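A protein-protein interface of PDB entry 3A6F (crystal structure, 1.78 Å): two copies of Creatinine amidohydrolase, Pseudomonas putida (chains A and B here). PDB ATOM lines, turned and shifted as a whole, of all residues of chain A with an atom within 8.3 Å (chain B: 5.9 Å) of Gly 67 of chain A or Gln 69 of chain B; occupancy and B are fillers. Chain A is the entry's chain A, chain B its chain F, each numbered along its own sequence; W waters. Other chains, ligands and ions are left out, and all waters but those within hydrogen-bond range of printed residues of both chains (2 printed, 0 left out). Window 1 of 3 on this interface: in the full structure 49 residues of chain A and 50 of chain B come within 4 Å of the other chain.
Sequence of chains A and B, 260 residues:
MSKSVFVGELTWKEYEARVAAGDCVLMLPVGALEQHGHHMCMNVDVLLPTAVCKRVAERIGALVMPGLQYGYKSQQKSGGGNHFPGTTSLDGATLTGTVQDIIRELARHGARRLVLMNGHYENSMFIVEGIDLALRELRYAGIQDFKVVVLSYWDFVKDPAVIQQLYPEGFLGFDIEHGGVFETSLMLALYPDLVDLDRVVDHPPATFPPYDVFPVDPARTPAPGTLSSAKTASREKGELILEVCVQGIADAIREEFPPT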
ATOM      1  N   PHE A   6     -25.881 -26.118 -21.816  1.00  0.00           N
ATOM      2  CA  PHE A   6     -25.609 -26.245 -20.386  1.00  0.00           C
ATOM      3  C   PHE A   6     -26.868 -26.515 -19.570  1.00  0.00           C
ATOM      4  O   PHE A   6     -27.807 -25.703 -19.546  1.00  0.00           O
ATOM      5  CB  PHE A   6     -24.906 -24.986 -19.857  1.00  0.00           C
ATOM      6  CG  PHE A   6     -23.557 -24.744 -20.473  1.00  0.00           C
ATOM      7  CD1 PHE A   6     -23.383 -23.755 -21.440  1.00  0.00           C
ATOM      8  CD2 PHE A   6     -22.466 -25.534 -20.117  1.00  0.00           C
ATOM      9  CE1 PHE A   6     -22.146 -23.557 -22.044  1.00  0.00           C
ATOM     10  CE2 PHE A   6     -21.222 -25.346 -20.714  1.00  0.00           C
ATOM     11  CZ  PHE A   6     -21.059 -24.355 -21.682  1.00  0.00           C
ATOM     12  N   GLY A   8     -27.330 -26.426 -16.419  1.00  0.00           N
ATOM     13  CA  GLY A   8     -27.595 -25.413 -15.416  1.00  0.00           C
ATOM     14  C   GLY A   8     -28.443 -24.256 -15.937  1.00  0.00           C
ATOM     15  O   GLY A   8     -29.180 -23.638 -15.177  1.00  0.00           O
ATOM     16  N   MET A  27     -22.958 -34.732 -20.621  1.00  0.00           N
ATOM     17  CA  MET A  27     -21.512 -34.627 -20.502  1.00  0.00           C
ATOM     18  C   MET A  27     -21.182 -33.941 -19.173  1.00  0.00           C
ATOM     19  O   MET A  27     -21.842 -32.986 -18.780  1.00  0.00           O
ATOM     20  CB  MET A  27     -20.950 -33.811 -21.671  1.00  0.00           C
ATOM     21  CG  MET A  27     -21.343 -34.360 -23.047  1.00  0.00           C
ATOM     22  SD  MET A  27     -20.654 -33.387 -24.408  1.00  0.00           S
ATOM     23  CE  MET A  27     -18.980 -34.065 -24.485  1.00  0.00           C
ATOM     24  N   LEU A  28     -20.158 -34.433 -18.487  1.00  0.00           N
ATOM     25  CA  LEU A  28     -19.764 -33.863 -17.205  1.00  0.00           C
ATOM     26  C   LEU A  28     -18.274 -33.565 -17.155  1.00  0.00           C
ATOM     27  O   LEU A  28     -17.447 -34.479 -17.117  1.00  0.00           O
ATOM     28  CB  LEU A  28     -20.133 -34.818 -16.063  1.00  0.00           C
ATOM     29  CG  LEU A  28     -19.629 -34.480 -14.652  1.00  0.00           C
ATOM     30  CD1 LEU A  28     -20.217 -33.163 -14.190  1.00  0.00           C
ATOM     31  CD2 LEU A  28     -20.016 -35.596 -13.689  1.00  0.00           C
ATOM     32  N   PRO A  29     -17.912 -32.274 -17.169  1.00  0.00           N
ATOM     33  CA  PRO A  29     -16.511 -31.853 -17.115  1.00  0.00           C
ATOM     34  C   PRO A  29     -15.979 -32.071 -15.703  1.00  0.00           C
ATOM     35  O   PRO A  29     -16.675 -31.781 -14.731  1.00  0.00           O
ATOM     36  CB  PRO A  29     -16.575 -30.356 -17.450  1.00  0.00           C
ATOM     37  CG  PRO A  29     -17.914 -30.181 -18.136  1.00  0.00           C
ATOM     38  CD  PRO A  29     -18.806 -31.128 -17.399  1.00  0.00           C
ATOM     39  N   VAL A  30     -14.758 -32.588 -15.583  1.00  0.00           N
ATOM     40  CA  VAL A  30     -14.165 -32.793 -14.267  1.00  0.00           C
ATOM     41  C   VAL A  30     -12.799 -32.130 -14.293  1.00  0.00           C
ATOM     42  O   VAL A  30     -11.893 -32.580 -15.001  1.00  0.00           O
ATOM     43  CB  VAL A  30     -14.004 -34.296 -13.933  1.00  0.00           C
ATOM     44  CG1 VAL A  30     -13.532 -34.461 -12.490  1.00  0.00           C
ATOM     45  CG2 VAL A  30     -15.329 -35.016 -14.126  1.00  0.00           C
ATOM     46  N   GLY A  31     -12.656 -31.050 -13.530  1.00  0.00           N
ATOM     47  CA  GLY A  31     -11.394 -30.327 -13.523  1.00  0.00           C
ATOM     48  C   GLY A  31     -10.658 -30.255 -12.200  1.00  0.00           C
ATOM     49  O   GLY A  31     -10.553 -31.248 -11.468  1.00  0.00           O
ATOM     50  N   ALA A  32     -10.147 -29.067 -11.899  1.00  0.00           N
ATOM     51  CA  ALA A  32      -9.401 -28.836 -10.678  1.00  0.00           C
ATOM     52  C   ALA A  32      -9.029 -27.365 -10.553  1.00  0.00           C
ATOM     53  O   ALA A  32      -9.134 -26.611 -11.514  1.00  0.00           O
ATOM     54  CB  ALA A  32      -8.120 -29.683 -10.691  1.00  0.00           C
ATOM     55  N   ASP A  45      -7.902 -26.363 -15.748  1.00  0.00           N
ATOM     56  CA  ASP A  45      -8.465 -27.710 -15.869  1.00  0.00           C
ATOM     57  C   ASP A  45      -9.978 -27.807 -15.866  1.00  0.00           C
ATOM     58  O   ASP A  45     -10.536 -28.876 -16.125  1.00  0.00           O
ATOM     59  CB  ASP A  45      -7.885 -28.621 -14.801  1.00  0.00           C
ATOM     60  CG  ASP A  45      -6.401 -28.813 -14.978  1.00  0.00           C
ATOM     61  OD1 ASP A  45      -5.913 -28.490 -16.082  1.00  0.00           O
ATOM     62  OD2 ASP A  45      -5.733 -29.284 -14.043  1.00  0.00           O
ATOM     63  N   VAL A  46     -10.637 -26.697 -15.563  1.00  0.00           N
ATOM     64  CA  VAL A  46     -12.088 -26.644 -15.572  1.00  0.00           C
ATOM     65  C   VAL A  46     -12.492 -25.992 -16.886  1.00  0.00           C
ATOM     66  O   VAL A  46     -13.351 -26.495 -17.611  1.00  0.00           O
ATOM     67  CB  VAL A  46     -12.637 -25.789 -14.412  1.00  0.00           C
ATOM     68  CG1 VAL A  46     -14.139 -25.633 -14.554  1.00  0.00           C
ATOM     69  CG2 VAL A  46     -12.293 -26.432 -13.080  1.00  0.00           C
ATOM     70  N   PRO A  49     -11.799 -28.490 -20.434  1.00  0.00           N
ATOM     71  CA  PRO A  49     -12.752 -29.554 -20.775  1.00  0.00           C
ATOM     72  C   PRO A  49     -14.180 -29.021 -20.969  1.00  0.00           C
ATOM     73  O   PRO A  49     -14.967 -29.602 -21.718  1.00  0.00           O
ATOM     74  CB  PRO A  49     -12.638 -30.514 -19.592  1.00  0.00           C
ATOM     75  CG  PRO A  49     -12.300 -29.591 -18.442  1.00  0.00           C
ATOM     76  CD  PRO A  49     -11.279 -28.653 -19.065  1.00  0.00           C
ATOM     77  N   THR A  50     -14.512 -27.921 -20.299  1.00  0.00           N
ATOM     78  CA  THR A  50     -15.848 -27.337 -20.433  1.00  0.00           C
ATOM     79  C   THR A  50     -16.025 -26.726 -21.828  1.00  0.00           C
ATOM     80  O   THR A  50     -17.088 -26.850 -22.443  1.00  0.00           O
ATOM     81  CB  THR A  50     -16.091 -26.250 -19.370  1.00  0.00           C
ATOM     82  OG1 THR A  50     -15.922 -26.816 -18.064  1.00  0.00           O
ATOM     83  CG2 THR A  50     -17.515 -25.692 -19.486  1.00  0.00           C
ATOM     84  N   CYS A  53     -16.473 -29.559 -24.226  1.00  0.00           N
ATOM     85  CA  CYS A  53     -17.816 -30.112 -24.047  1.00  0.00           C
ATOM     86  C   CYS A  53     -18.875 -29.237 -24.708  1.00  0.00           C
ATOM     87  O   CYS A  53     -19.815 -29.740 -25.331  1.00  0.00           O
ATOM     88  CB  CYS A  53     -18.163 -30.240 -22.551  1.00  0.00           C
ATOM     89  SG  CYS A  53     -17.478 -31.678 -21.687  1.00  0.00           S
ATOM     90  N   VAL A  64     -24.519 -30.390 -21.344  1.00  0.00           N
ATOM     91  CA  VAL A  64     -23.364 -30.346 -20.455  1.00  0.00           C
ATOM     92  C   VAL A  64     -23.746 -30.007 -19.004  1.00  0.00           C
ATOM     93  O   VAL A  64     -24.344 -28.962 -18.739  1.00  0.00           O
ATOM     94  CB  VAL A  64     -22.335 -29.296 -20.956  1.00  0.00           C
ATOM     95  CG1 VAL A  64     -21.074 -29.337 -20.090  1.00  0.00           C
ATOM     96  CG2 VAL A  64     -21.980 -29.565 -22.427  1.00  0.00           C
ATOM     97  N   MET A  65     -23.400 -30.908 -18.085  1.00  0.00           N
ATOM     98  CA  MET A  65     -23.658 -30.744 -16.647  1.00  0.00           C
ATOM     99  C   MET A  65     -22.678 -29.732 -16.038  1.00  0.00           C
ATOM    100  O   MET A  65     -21.641 -29.417 -16.638  1.00  0.00           O
ATOM    101  CB  MET A  65     -23.451 -32.078 -15.916  1.00  0.00           C
ATOM    102  CG  MET A  65     -24.464 -33.183 -16.202  1.00  0.00           C
ATOM    103  SD  MET A  65     -26.119 -32.773 -15.635  1.00  0.00           S
ATOM    104  CE  MET A  65     -25.968 -32.948 -13.841  1.00  0.00           C
ATOM    105  N   PRO A  66     -23.005 -29.187 -14.851  1.00  0.00           N
ATOM    106  CA  PRO A  66     -22.092 -28.231 -14.217  1.00  0.00           C
ATOM    107  C   PRO A  66     -20.790 -28.990 -13.970  1.00  0.00           C
ATOM    108  O   PRO A  66     -20.820 -30.154 -13.582  1.00  0.00           O
ATOM    109  CB  PRO A  66     -22.808 -27.888 -12.915  1.00  0.00           C
ATOM    110  CG  PRO A  66     -24.248 -27.889 -13.340  1.00  0.00           C
ATOM    111  CD  PRO A  66     -24.334 -29.147 -14.206  1.00  0.00           C
ATOM    112  N   GLY A  67     -19.655 -28.342 -14.189  1.00  0.00           N
ATOM    113  CA  GLY A  67     -18.387 -29.036 -14.009  1.00  0.00           C
ATOM    114  C   GLY A  67     -17.915 -29.134 -12.575  1.00  0.00           C
ATOM    115  O   GLY A  67     -18.270 -28.303 -11.746  1.00  0.00           O
ATOM    116  N   LEU A  68     -17.132 -30.166 -12.270  1.00  0.00           N
ATOM    117  CA  LEU A  68     -16.596 -30.318 -10.923  1.00  0.00           C
ATOM    118  C   LEU A  68     -15.389 -29.387 -10.920  1.00  0.00           C
ATOM    119  O   LEU A  68     -14.482 -29.533 -11.746  1.00  0.00           O
ATOM    120  CB  LEU A  68     -16.182 -31.774 -10.664  1.00  0.00           C
ATOM    121  CG  LEU A  68     -17.344 -32.771 -10.794  1.00  0.00           C
ATOM    122  CD1 LEU A  68     -16.916 -34.136 -10.280  1.00  0.00           C
ATOM    123  CD2 LEU A  68     -18.545 -32.278 -10.000  1.00  0.00           C
ATOM    124  N   GLN A  69     -15.397 -28.431  -9.995  1.00  0.00           N
ATOM    125  CA  GLN A  69     -14.347 -27.417  -9.905  1.00  0.00           C
ATOM    126  C   GLN A  69     -13.092 -27.844  -9.146  1.00  0.00           C
ATOM    127  O   GLN A  69     -12.018 -27.260  -9.334  1.00  0.00           O
ATOM    128  CB  GLN A  69     -14.909 -26.159  -9.237  1.00  0.00           C
ATOM    129  CG  GLN A  69     -16.302 -25.729  -9.708  1.00  0.00           C
ATOM    130  CD  GLN A  69     -16.320 -25.229 -11.139  1.00  0.00           C
ATOM    131  OE1 GLN A  69     -17.001 -25.793 -12.001  1.00  0.00           O
ATOM    132  NE2 GLN A  69     -15.575 -24.164 -11.399  1.00  0.00           N
ATOM    133  N   TYR A  70     -13.231 -28.842  -8.276  1.00  0.00           N
ATOM    134  CA  TYR A  70     -12.107 -29.308  -7.472  1.00  0.00           C
ATOM    135  C   TYR A  70     -11.764 -30.755  -7.783  1.00  0.00           C
ATOM    136  O   TYR A  70     -12.653 -31.609  -7.869  1.00  0.00           O
ATOM    137  CB  TYR A  70     -12.432 -29.149  -5.976  1.00  0.00           C
ATOM    138  CG  TYR A  70     -12.735 -27.718  -5.562  1.00  0.00           C
ATOM    139  CD1 TYR A  70     -14.023 -27.186  -5.685  1.00  0.00           C
ATOM    140  CD2 TYR A  70     -11.721 -26.883  -5.084  1.00  0.00           C
ATOM    141  CE1 TYR A  70     -14.290 -25.853  -5.342  1.00  0.00           C
ATOM    142  CE2 TYR A  70     -11.976 -25.560  -4.745  1.00  0.00           C
ATOM    143  CZ  TYR A  70     -13.256 -25.051  -4.876  1.00  0.00           C
ATOM    144  OH  TYR A  70     -13.485 -23.733  -4.559  1.00  0.00           O
ATOM    145  N   THR A  98     -18.574 -37.763  -5.116  1.00  0.00           N
ATOM    146  CA  THR A  98     -19.299 -36.760  -5.881  1.00  0.00           C
ATOM    147  C   THR A  98     -19.743 -37.349  -7.229  1.00  0.00           C
ATOM    148  O   THR A  98     -20.884 -37.156  -7.665  1.00  0.00           O
ATOM    149  CB  THR A  98     -18.417 -35.512  -6.149  1.00  0.00           C
ATOM    150  OG1 THR A  98     -18.061 -34.895  -4.900  1.00  0.00           O
ATOM    151  CG2 THR A  98     -19.172 -34.511  -7.014  1.00  0.00           C
ATOM    152  N   ILE A 102     -23.741 -38.067  -8.477  1.00  0.00           N
ATOM    153  CA  ILE A 102     -24.291 -37.497  -9.699  1.00  0.00           C
ATOM    154  C   ILE A 102     -24.855 -38.584 -10.622  1.00  0.00           C
ATOM    155  O   ILE A 102     -25.963 -38.446 -11.155  1.00  0.00           O
ATOM    156  CB  ILE A 102     -23.223 -36.628 -10.421  1.00  0.00           C
ATOM    157  CG1 ILE A 102     -22.953 -35.370  -9.581  1.00  0.00           C
ATOM    158  CG2 ILE A 102     -23.685 -36.256 -11.818  1.00  0.00           C
ATOM    159  CD1 ILE A 102     -21.879 -34.444 -10.120  1.00  0.00           C
ATOM    160  N   MET A 117     -15.777 -36.016 -19.035  1.00  0.00           N
ATOM    161  CA  MET A 117     -14.584 -35.481 -19.668  1.00  0.00           C
ATOM    162  C   MET A 117     -13.648 -34.902 -18.627  1.00  0.00           C
ATOM    163  O   MET A 117     -13.910 -33.850 -18.052  1.00  0.00           O
ATOM    164  CB  MET A 117     -14.930 -34.397 -20.689  1.00  0.00           C
ATOM    165  CG  MET A 117     -13.774 -34.113 -21.643  1.00  0.00           C
ATOM    166  SD  MET A 117     -14.071 -32.769 -22.794  1.00  0.00           S
ATOM    167  CE  MET A 117     -15.372 -33.497 -23.823  1.00  0.00           C
ATOM    168  N   PRO B  29     -18.793 -19.867  -2.361  1.00  0.00           N
ATOM    169  CA  PRO B  29     -20.226 -19.990  -2.667  1.00  0.00           C
ATOM    170  C   PRO B  29     -20.579 -21.485  -2.659  1.00  0.00           C
ATOM    171  O   PRO B  29     -19.837 -22.288  -3.210  1.00  0.00           O
ATOM    172  CB  PRO B  29     -20.338 -19.408  -4.082  1.00  0.00           C
ATOM    173  CG  PRO B  29     -19.107 -18.544  -4.222  1.00  0.00           C
ATOM    174  CD  PRO B  29     -18.056 -19.375  -3.538  1.00  0.00           C
ATOM    175  N   GLY B  31     -23.732 -23.851  -3.703  1.00  0.00           N
ATOM    176  CA  GLY B  31     -25.060 -23.866  -4.283  1.00  0.00           C
ATOM    177  C   GLY B  31     -25.711 -25.213  -4.485  1.00  0.00           C
ATOM    178  O   GLY B  31     -25.717 -26.057  -3.588  1.00  0.00           O
ATOM    179  N   ALA B  32     -26.273 -25.401  -5.677  1.00  0.00           N
ATOM    180  CA  ALA B  32     -26.951 -26.641  -6.020  1.00  0.00           C
ATOM    181  C   ALA B  32     -27.463 -26.586  -7.452  1.00  0.00           C
ATOM    182  O   ALA B  32     -27.509 -25.519  -8.072  1.00  0.00           O
ATOM    183  CB  ALA B  32     -28.121 -26.861  -5.082  1.00  0.00           C
ATOM    184  N   LEU B  33     -27.830 -27.752  -7.968  1.00  0.00           N
ATOM    185  CA  LEU B  33     -28.413 -27.858  -9.294  1.00  0.00           C
ATOM    186  C   LEU B  33     -29.778 -28.365  -8.885  1.00  0.00           C
ATOM    187  O   LEU B  33     -29.929 -29.527  -8.497  1.00  0.00           O
ATOM    188  CB  LEU B  33     -27.678 -28.878 -10.163  1.00  0.00           C
ATOM    189  CG  LEU B  33     -28.219 -28.981 -11.596  1.00  0.00           C
ATOM    190  CD1 LEU B  33     -28.094 -27.630 -12.294  1.00  0.00           C
ATOM    191  CD2 LEU B  33     -27.456 -30.045 -12.361  1.00  0.00           C
ATOM    192  N   VAL B  46     -26.450 -21.499  -7.380  1.00  0.00           N
ATOM    193  CA  VAL B  46     -25.014 -21.289  -7.524  1.00  0.00           C
ATOM    194  C   VAL B  46     -24.821 -19.837  -7.995  1.00  0.00           C
ATOM    195  O   VAL B  46     -24.006 -19.086  -7.451  1.00  0.00           O
ATOM    196  CB  VAL B  46     -24.391 -22.241  -8.587  1.00  0.00           C
ATOM    197  CG1 VAL B  46     -22.965 -21.803  -8.907  1.00  0.00           C
ATOM    198  CG2 VAL B  46     -24.398 -23.672  -8.077  1.00  0.00           C
ATOM    199  N   PRO B  66     -13.870 -21.047  -6.334  1.00  0.00           N
ATOM    200  CA  PRO B  66     -14.851 -21.620  -7.264  1.00  0.00           C
ATOM    201  C   PRO B  66     -16.020 -22.160  -6.430  1.00  0.00           C
ATOM    202  O   PRO B  66     -15.806 -22.804  -5.402  1.00  0.00           O
ATOM    203  CB  PRO B  66     -14.060 -22.728  -7.955  1.00  0.00           C
ATOM    204  CG  PRO B  66     -12.649 -22.179  -7.955  1.00  0.00           C
ATOM    205  CD  PRO B  66     -12.532 -21.630  -6.547  1.00  0.00           C
ATOM    206  N   GLY B  67     -17.248 -21.891  -6.863  1.00  0.00           N
ATOM    207  CA  GLY B  67     -18.401 -22.341  -6.103  1.00  0.00           C
ATOM    208  C   GLY B  67     -18.758 -23.817  -6.209  1.00  0.00           C
ATOM    209  O   GLY B  67     -18.509 -24.459  -7.226  1.00  0.00           O
ATOM    210  N   LEU B  68     -19.331 -24.362  -5.143  1.00  0.00           N
ATOM    211  CA  LEU B  68     -19.754 -25.762  -5.144  1.00  0.00           C
ATOM    212  C   LEU B  68     -21.056 -25.805  -5.939  1.00  0.00           C
ATOM    213  O   LEU B  68     -22.069 -25.226  -5.530  1.00  0.00           O
ATOM    214  CB  LEU B  68     -19.969 -26.251  -3.710  1.00  0.00           C
ATOM    215  CG  LEU B  68     -18.704 -26.178  -2.846  1.00  0.00           C
ATOM    216  CD1 LEU B  68     -18.960 -26.862  -1.511  1.00  0.00           C
ATOM    217  CD2 LEU B  68     -17.535 -26.851  -3.575  1.00  0.00           C
ATOM    218  N   GLN B  69     -21.004 -26.471  -7.088  1.00  0.00           N
ATOM    219  CA  GLN B  69     -22.139 -26.582  -8.001  1.00  0.00           C
ATOM    220  C   GLN B  69     -23.242 -27.541  -7.562  1.00  0.00           C
ATOM    221  O   GLN B  69     -24.397 -27.385  -7.964  1.00  0.00           O
ATOM    222  CB  GLN B  69     -21.641 -27.024  -9.386  1.00  0.00           C
ATOM    223  CG  GLN B  69     -20.380 -26.314  -9.871  1.00  0.00           C
ATOM    224  CD  GLN B  69     -20.642 -24.896 -10.324  1.00  0.00           C
ATOM    225  OE1 GLN B  69     -21.440 -24.665 -11.227  1.00  0.00           O
ATOM    226  NE2 GLN B  69     -19.959 -23.934  -9.705  1.00  0.00           N
ATOM    227  N   TYR B  70     -22.893 -28.542  -6.762  1.00  0.00           N
ATOM    228  CA  TYR B  70     -23.877 -29.523  -6.312  1.00  0.00           C
ATOM    229  C   TYR B  70     -24.077 -29.473  -4.799  1.00  0.00           C
ATOM    230  O   TYR B  70     -23.109 -29.441  -4.043  1.00  0.00           O
ATOM    231  CB  TYR B  70     -23.445 -30.921  -6.749  1.00  0.00           C
ATOM    232  CG  TYR B  70     -23.302 -31.062  -8.249  1.00  0.00           C
ATOM    233  CD1 TYR B  70     -22.096 -30.782  -8.883  1.00  0.00           C
ATOM    234  CD2 TYR B  70     -24.385 -31.459  -9.037  1.00  0.00           C
ATOM    235  CE1 TYR B  70     -21.960 -30.892 -10.266  1.00  0.00           C
ATOM    236  CE2 TYR B  70     -24.262 -31.570 -10.429  1.00  0.00           C
ATOM    237  CZ  TYR B  70     -23.051 -31.289 -11.032  1.00  0.00           C
ATOM    238  OH  TYR B  70     -22.913 -31.420 -12.400  1.00  0.00           O
ATOM    239  N   GLY B  71     -25.335 -29.469  -4.366  1.00  0.00           N
ATOM    240  CA  GLY B  71     -25.634 -29.390  -2.942  1.00  0.00           C
ATOM    241  C   GLY B  71     -26.450 -30.553  -2.412  1.00  0.00           C
ATOM    242  O   GLY B  71     -26.737 -31.490  -3.151  1.00  0.00           O
ATOM    243  N   THR B  88     -30.032 -32.435  -9.095  1.00  0.00           N
ATOM    244  CA  THR B  88     -28.977 -33.446  -8.975  1.00  0.00           C
ATOM    245  C   THR B  88     -28.270 -33.185  -7.652  1.00  0.00           C
ATOM    246  O   THR B  88     -27.456 -32.269  -7.544  1.00  0.00           O
ATOM    247  CB  THR B  88     -28.010 -33.306 -10.161  1.00  0.00           C
ATOM    248  OG1 THR B  88     -28.763 -33.395 -11.379  1.00  0.00           O
ATOM    249  CG2 THR B  88     -26.958 -34.403 -10.146  1.00  0.00           C
HETATM  250  O   HOH W   1     -20.288 -25.079 -13.940  1.00  0.00           O
HETATM  251  O   HOH W   2     -16.805 -21.563 -10.076  1.00  0.00           O
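OH of Tyr 70 of chain B is in hydrogen-bond range of O of Pro 66 of chain A, at 2.7 Å. The side-chain hydroxyl (OH) of Tyr 70 of chain A sits at hydrogen-bond distance from the backbone carbonyl oxygen (O) of Pro 66 of chain B, 2.6 Å away.
The backbone NH of Gly 31 of chain A lies within hydrogen-bond range of the backbone carbonyl oxygen of Leu 68 of chain A, at 3.0 Å. N of Leu 68 of chain B is in hydrogen-bond range of O of Pro 29 of chain B, 2.9 Å away. The backbone carbonyl oxygen (O) of Leu 68 of chain B lies within hydrogen-bond range of the backbone NH (N) of Gly 31 of chain B (2.8 Å). N of Leu 33 of chain B sits at hydrogen-bond distance from O of Gln 69 of chain B. The backbone carbonyl oxygen (O) of Leu 33 of chain B sits at hydrogen-bond distance from the backbone NH (N) of Thr 88 of chain B, 3.0 Å away. The backbone carbonyl oxygen (O) of Gly 67 of chain B is in hydrogen-bond range of the side-chain amide nitrogen (NE2) of Gln 69 of chain B (2.9 Å).
Met 65 of chain A touches Leu 33 of chain B. Tyr 70 of chain B touches Met 65 of chain A. CE of Met 65 of chain A touches OG1 of Thr 88 of chain B (3.8 Å). CD of Pro 66 of chain A touches CD2 of Leu 33 of chain B, at 3.7 Å. CB of Gln 69 of chain B touches CB of Pro 66 of chain A, at 3.8 Å. CD2 of Leu 68 of chain A touches CE1 of Tyr 70 of chain B (3.7 Å). Pro 66 of chain B touches Gln 69 of chain A (CB to CB, 3.8 Å). CG of Gln 69 of chain A touches O of Gly 67 of chain B, at 3.6 Å. Tyr 70 of chain A touches Leu 68 of chain B (CE1 to CD2, 3.8 Å). Ile 102 of chain A touches Tyr 70 of chain B.
Printed residues of chain B within 4 Å of Leu 28 of chain A: Tyr 70. Of the printed residues of chain B, Met 65 of chain A touches Leu 33, Tyr 70 and Thr 88. Of the printed residues of chain B, Pro 66 of chain A touches Leu 33 (3.7 Å), Gln 69 (3.8 Å) and Tyr 70 (2.7 Å). Of the printed residues of chain B, Tyr 70 of chain A touches Pro 66 (2.6 Å) and Leu 68 (3.8 Å). Of the printed residues of chain A, Gln 69 of chain B touches Pro 66 (3.8 Å) and Gly 67 (3.5 Å). Printed residues of chain A within 4 Å of Tyr 70 of chain B: Leu 28 (3.7 Å), Met 65 (3.6 Å), Pro 66 (2.7 Å), Leu 68 (3.7 Å) and Ile 102 (3.5 Å). The nearest residue of chain B that does not touch Gly 67 of chain A is Tyr 70 of chain B (4.7 Å).
Hydrophobic or aromatic side chains of chain B within 4 Å of the printed part of chain A: Leu 33, Pro 66, Leu 68 and Tyr 70. Along chain B the printed residues that touch a printed residue of chain A span positions 33 to 88. Among the printed residues, no Asp or Glu carboxylate lies within 4 Å of a Lys or Arg side-chain nitrogen of the other chain.
Pro 66 of chain A touches Gln 69 of chain B, and with the chains exchanged Gln 69 of chain A touches Pro 66 of chain B. Pro 66 of chain A touches Tyr 70 of chain B, and with the chains exchanged Tyr 70 of chain A touches Pro 66 of chain B. Gly 67 of chain A touches Gln 69 of chain B, and with the chains exchanged Gln 69 of chain A touches Gly 67 of chain B. Leu 68 of chain A touches Tyr 70 of chain B, and with the chains exchanged Tyr 70 of chain A touches Leu 68 of chain B.
Water W1 lies within hydrogen-bond range of OE1 of Gln 69 of chain B (3.0 Å) and N of Gly 67 of chain A (3.3 Å). Water W2 lies within hydrogen-bond range of the side-chain amide nitrogen (NE2) of Gln 69 of chain A and the backbone NH (N) of Gly 67 of chain B.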
